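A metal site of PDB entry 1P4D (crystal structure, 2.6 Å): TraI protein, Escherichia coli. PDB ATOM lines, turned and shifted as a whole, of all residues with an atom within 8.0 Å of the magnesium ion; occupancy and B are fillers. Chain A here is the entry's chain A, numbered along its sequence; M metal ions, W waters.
Water W3 binds the magnesium ion.
Water W1 is bound to the magnesium ion.
A ring nitrogen (NE2) of His 159 binds the magnesium ion, at 2.2 Å.
The magnesium ion is bound by water W2 (2.2 Å).
NE2 of His 157 binds the magnesium ion, 2.3 Å away.
A ring nitrogen (ND1) of His 146 is bound to the magnesium ion (2.5 Å).
The side-chain carboxylate (OD2) of Asp 81 is in hydrogen-bond range of a ring nitrogen (ND1) of His 159, 3.0 Å away.
ND1 of His 157 sits at hydrogen-bond distance from O of Gln 155, at 2.9 Å.
OG1 of Thr 83 sits at hydrogen-bond distance from ND1 of His 159 (3.1 Å).
The backbone NH (N) of His 159 sits at hydrogen-bond distance from the backbone carbonyl oxygen (O) of Phe 144 (2.9 Å).
A ring nitrogen (NE2) of His 146 sits at hydrogen-bond distance from the backbone carbonyl oxygen of Tyr 17 (3.1 Å).
Of the 16 residues printed, 3 come within 4 Å of the magnesium ion.
The nearest printed residue that does not touch the magnesium ion is Thr 148 (4.8 Å).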
ATOM      1  N   TYR A  16     -23.348  -4.886  10.483  1.00  0.00           N
ATOM      2  CA  TYR A  16     -22.725  -4.543   9.220  1.00  0.00           C
ATOM      3  C   TYR A  16     -21.242  -4.200   9.392  1.00  0.00           C
ATOM      4  O   TYR A  16     -20.409  -4.589   8.575  1.00  0.00           O
ATOM      5  CB  TYR A  16     -23.438  -3.367   8.573  1.00  0.00           C
ATOM      6  CG  TYR A  16     -22.659  -2.735   7.449  1.00  0.00           C
ATOM      7  CD1 TYR A  16     -22.543  -3.357   6.207  1.00  0.00           C
ATOM      8  CD2 TYR A  16     -22.018  -1.500   7.632  1.00  0.00           C
ATOM      9  CE1 TYR A  16     -21.830  -2.755   5.168  1.00  0.00           C
ATOM     10  CE2 TYR A  16     -21.305  -0.905   6.600  1.00  0.00           C
ATOM     11  CZ  TYR A  16     -21.211  -1.533   5.368  1.00  0.00           C
ATOM     12  OH  TYR A  16     -20.508  -0.927   4.363  1.00  0.00           O
ATOM     13  N   TYR A  17     -20.909  -3.455  10.445  1.00  0.00           N
ATOM     14  CA  TYR A  17     -19.525  -3.065  10.669  1.00  0.00           C
ATOM     15  C   TYR A  17     -18.736  -4.081  11.481  1.00  0.00           C
ATOM     16  O   TYR A  17     -17.516  -4.041  11.488  1.00  0.00           O
ATOM     17  CB  TYR A  17     -19.433  -1.713  11.408  1.00  0.00           C
ATOM     18  CG  TYR A  17     -19.900  -0.496  10.623  1.00  0.00           C
ATOM     19  CD1 TYR A  17     -21.169   0.038  10.809  1.00  0.00           C
ATOM     20  CD2 TYR A  17     -19.073   0.092   9.653  1.00  0.00           C
ATOM     21  CE1 TYR A  17     -21.616   1.114  10.050  1.00  0.00           C
ATOM     22  CE2 TYR A  17     -19.517   1.169   8.881  1.00  0.00           C
ATOM     23  CZ  TYR A  17     -20.782   1.675   9.081  1.00  0.00           C
ATOM     24  OH  TYR A  17     -21.237   2.720   8.304  1.00  0.00           O
ATOM     25  N   ASN A  22     -15.896  -9.535   7.881  1.00  0.00           N
ATOM     26  CA  ASN A  22     -15.341  -8.322   7.267  1.00  0.00           C
ATOM     27  C   ASN A  22     -13.872  -8.149   7.593  1.00  0.00           C
ATOM     28  O   ASN A  22     -13.189  -7.318   6.995  1.00  0.00           O
ATOM     29  CB  ASN A  22     -16.090  -7.074   7.734  1.00  0.00           C
ATOM     30  CG  ASN A  22     -17.526  -7.027   7.259  1.00  0.00           C
ATOM     31  OD1 ASN A  22     -17.810  -7.278   6.083  1.00  0.00           O
ATOM     32  ND2 ASN A  22     -18.439  -6.710   8.177  1.00  0.00           N
ATOM     33  N   ASP A  81     -19.971   7.867   7.690  1.00  0.00           N
ATOM     34  CA  ASP A  81     -18.951   6.859   7.509  1.00  0.00           C
ATOM     35  C   ASP A  81     -17.807   7.421   6.662  1.00  0.00           C
ATOM     36  O   ASP A  81     -17.969   7.655   5.467  1.00  0.00           O
ATOM     37  CB  ASP A  81     -19.553   5.631   6.811  1.00  0.00           C
ATOM     38  CG  ASP A  81     -18.573   4.475   6.737  1.00  0.00           C
ATOM     39  OD1 ASP A  81     -17.368   4.714   6.548  1.00  0.00           O
ATOM     40  OD2 ASP A  81     -19.014   3.316   6.828  1.00  0.00           O
ATOM     41  N   THR A  83     -14.510   6.412   5.204  1.00  0.00           N
ATOM     42  CA  THR A  83     -13.712   5.222   4.911  1.00  0.00           C
ATOM     43  C   THR A  83     -12.316   5.464   4.331  1.00  0.00           C
ATOM     44  O   THR A  83     -12.195   5.962   3.215  1.00  0.00           O
ATOM     45  CB  THR A  83     -14.451   4.270   3.913  1.00  0.00           C
ATOM     46  OG1 THR A  83     -15.759   3.948   4.394  1.00  0.00           O
ATOM     47  CG2 THR A  83     -13.660   2.984   3.752  1.00  0.00           C
ATOM     48  N   PHE A 144     -13.437   0.652  12.546  1.00  0.00           N
ATOM     49  CA  PHE A 144     -13.417  -0.777  12.301  1.00  0.00           C
ATOM     50  C   PHE A 144     -12.579  -1.095  11.039  1.00  0.00           C
ATOM     51  O   PHE A 144     -12.789  -0.514   9.974  1.00  0.00           O
ATOM     52  CB  PHE A 144     -14.847  -1.318  12.124  1.00  0.00           C
ATOM     53  CG  PHE A 144     -15.845  -0.803  13.134  1.00  0.00           C
ATOM     54  CD1 PHE A 144     -16.481   0.425  12.943  1.00  0.00           C
ATOM     55  CD2 PHE A 144     -16.189  -1.572  14.235  1.00  0.00           C
ATOM     56  CE1 PHE A 144     -17.442   0.876  13.828  1.00  0.00           C
ATOM     57  CE2 PHE A 144     -17.163  -1.131  15.138  1.00  0.00           C
ATOM     58  CZ  PHE A 144     -17.796   0.098  14.933  1.00  0.00           C
ATOM     59  N   ASN A 145     -11.629  -2.008  11.174  1.00  0.00           N
ATOM     60  CA  ASN A 145     -10.783  -2.403  10.047  1.00  0.00           C
ATOM     61  C   ASN A 145     -11.415  -3.567   9.273  1.00  0.00           C
ATOM     62  O   ASN A 145     -11.885  -4.547   9.855  1.00  0.00           O
ATOM     63  CB  ASN A 145      -9.380  -2.824  10.538  1.00  0.00           C
ATOM     64  CG  ASN A 145      -8.583  -1.662  11.117  1.00  0.00           C
ATOM     65  OD1 ASN A 145      -7.526  -1.850  11.729  1.00  0.00           O
ATOM     66  ND2 ASN A 145      -9.080  -0.441  10.929  1.00  0.00           N
ATOM     67  N   HIS A 146     -11.447  -3.439   7.965  1.00  0.00           N
ATOM     68  CA  HIS A 146     -11.968  -4.501   7.106  1.00  0.00           C
ATOM     69  C   HIS A 146     -10.811  -4.821   6.150  1.00  0.00           C
ATOM     70  O   HIS A 146      -9.823  -4.082   6.097  1.00  0.00           O
ATOM     71  CB  HIS A 146     -13.226  -4.023   6.353  1.00  0.00           C
ATOM     72  CG  HIS A 146     -14.435  -3.885   7.237  1.00  0.00           C
ATOM     73  ND1 HIS A 146     -15.686  -3.557   6.748  1.00  0.00           N
ATOM     74  CD2 HIS A 146     -14.582  -4.045   8.575  1.00  0.00           C
ATOM     75  CE1 HIS A 146     -16.553  -3.533   7.748  1.00  0.00           C
ATOM     76  NE2 HIS A 146     -15.911  -3.826   8.869  1.00  0.00           N
ATOM     77  N   ASP A 147     -10.936  -5.904   5.388  1.00  0.00           N
ATOM     78  CA  ASP A 147      -9.856  -6.302   4.483  1.00  0.00           C
ATOM     79  C   ASP A 147     -10.301  -6.647   3.068  1.00  0.00           C
ATOM     80  O   ASP A 147      -9.464  -6.977   2.212  1.00  0.00           O
ATOM     81  CB  ASP A 147      -9.127  -7.496   5.082  1.00  0.00           C
ATOM     82  CG  ASP A 147     -10.089  -8.620   5.484  1.00  0.00           C
ATOM     83  OD1 ASP A 147     -11.116  -8.798   4.794  1.00  0.00           O
ATOM     84  OD2 ASP A 147      -9.808  -9.322   6.478  1.00  0.00           O
ATOM     85  N   THR A 148     -11.591  -6.539   2.798  1.00  0.00           N
ATOM     86  CA  THR A 148     -12.115  -6.919   1.480  1.00  0.00           C
ATOM     87  C   THR A 148     -12.926  -5.849   0.739  1.00  0.00           C
ATOM     88  O   THR A 148     -13.836  -5.249   1.301  1.00  0.00           O
ATOM     89  CB  THR A 148     -12.974  -8.193   1.622  1.00  0.00           C
ATOM     90  OG1 THR A 148     -12.245  -9.175   2.385  1.00  0.00           O
ATOM     91  CG2 THR A 148     -13.346  -8.768   0.241  1.00  0.00           C
ATOM     92  N   SER A 149     -12.587  -5.632  -0.530  1.00  0.00           N
ATOM     93  CA  SER A 149     -13.275  -4.648  -1.379  1.00  0.00           C
ATOM     94  C   SER A 149     -14.651  -5.141  -1.824  1.00  0.00           C
ATOM     95  O   SER A 149     -15.076  -6.228  -1.485  1.00  0.00           O
ATOM     96  CB  SER A 149     -12.448  -4.369  -2.626  1.00  0.00           C
ATOM     97  OG  SER A 149     -12.531  -5.442  -3.567  1.00  0.00           O
ATOM     98  N   ARG A 150     -15.312  -4.310  -2.616  1.00  0.00           N
ATOM     99  CA  ARG A 150     -16.650  -4.611  -3.122  1.00  0.00           C
ATOM    100  C   ARG A 150     -16.595  -5.780  -4.094  1.00  0.00           C
ATOM    101  O   ARG A 150     -17.524  -6.585  -4.169  1.00  0.00           O
ATOM    102  CB  ARG A 150     -17.225  -3.385  -3.822  1.00  0.00           C
ATOM    103  CG  ARG A 150     -18.726  -3.233  -3.710  1.00  0.00           C
ATOM    104  CD  ARG A 150     -19.166  -1.950  -4.413  1.00  0.00           C
ATOM    105  NE  ARG A 150     -20.517  -1.539  -4.020  1.00  0.00           N
ATOM    106  CZ  ARG A 150     -21.097  -0.407  -4.429  1.00  0.00           C
ATOM    107  NH1 ARG A 150     -20.439   0.431  -5.235  1.00  0.00           N
ATOM    108  NH2 ARG A 150     -22.318  -0.100  -4.019  1.00  0.00           N
ATOM    109  N   GLN A 155      -8.276  -5.337   0.291  1.00  0.00           N
ATOM    110  CA  GLN A 155      -8.385  -3.903   0.501  1.00  0.00           C
ATOM    111  C   GLN A 155      -8.436  -3.562   1.997  1.00  0.00           C
ATOM    112  O   GLN A 155      -9.482  -3.647   2.630  1.00  0.00           O
ATOM    113  CB  GLN A 155      -9.629  -3.362  -0.201  1.00  0.00           C
ATOM    114  CG  GLN A 155      -9.622  -1.848  -0.243  1.00  0.00           C
ATOM    115  CD  GLN A 155     -10.839  -1.278  -0.915  1.00  0.00           C
ATOM    116  OE1 GLN A 155     -11.954  -1.389  -0.408  1.00  0.00           O
ATOM    117  NE2 GLN A 155     -10.633  -0.663  -2.070  1.00  0.00           N
ATOM    118  N   HIS A 157      -8.946  -1.393   4.929  1.00  0.00           N
ATOM    119  CA  HIS A 157      -9.587  -0.119   5.146  1.00  0.00           C
ATOM    120  C   HIS A 157     -10.155   0.021   6.534  1.00  0.00           C
ATOM    121  O   HIS A 157     -10.321  -0.952   7.258  1.00  0.00           O
ATOM    122  CB  HIS A 157     -10.675   0.175   4.068  1.00  0.00           C
ATOM    123  CG  HIS A 157     -11.808  -0.807   4.016  1.00  0.00           C
ATOM    124  ND1 HIS A 157     -11.740  -1.986   3.309  1.00  0.00           N
ATOM    125  CD2 HIS A 157     -13.064  -0.743   4.522  1.00  0.00           C
ATOM    126  CE1 HIS A 157     -12.909  -2.611   3.369  1.00  0.00           C
ATOM    127  NE2 HIS A 157     -13.726  -1.875   4.099  1.00  0.00           N
ATOM    128  N   THR A 158     -10.426   1.262   6.922  1.00  0.00           N
ATOM    129  CA  THR A 158     -11.012   1.520   8.217  1.00  0.00           C
ATOM    130  C   THR A 158     -12.226   2.380   8.004  1.00  0.00           C
ATOM    131  O   THR A 158     -12.131   3.422   7.369  1.00  0.00           O
ATOM    132  CB  THR A 158     -10.066   2.300   9.160  1.00  0.00           C
ATOM    133  OG1 THR A 158      -8.834   1.591   9.312  1.00  0.00           O
ATOM    134  CG2 THR A 158     -10.736   2.493  10.519  1.00  0.00           C
ATOM    135  N   HIS A 159     -13.379   1.930   8.506  1.00  0.00           N
ATOM    136  CA  HIS A 159     -14.603   2.707   8.425  1.00  0.00           C
ATOM    137  C   HIS A 159     -14.630   3.521   9.704  1.00  0.00           C
ATOM    138  O   HIS A 159     -14.838   2.970  10.797  1.00  0.00           O
ATOM    139  CB  HIS A 159     -15.823   1.798   8.437  1.00  0.00           C
ATOM    140  CG  HIS A 159     -16.048   1.043   7.168  1.00  0.00           C
ATOM    141  ND1 HIS A 159     -16.691   1.584   6.089  1.00  0.00           N
ATOM    142  CD2 HIS A 159     -15.729  -0.228   6.833  1.00  0.00           C
ATOM    143  CE1 HIS A 159     -16.773   0.686   5.129  1.00  0.00           C
ATOM    144  NE2 HIS A 159     -16.204  -0.427   5.558  1.00  0.00           N
HETATM  145 MG    MG M   1     -15.898  -2.379   4.530  1.00  0.00          MG
HETATM  146  O   HOH W   1     -15.791  -4.278   3.692  1.00  0.00           O
HETATM  147  O   HOH W   2     -18.102  -2.576   4.890  1.00  0.00           O
HETATM  148  O   HOH W   3     -16.331  -1.298   2.881  1.00  0.00           O
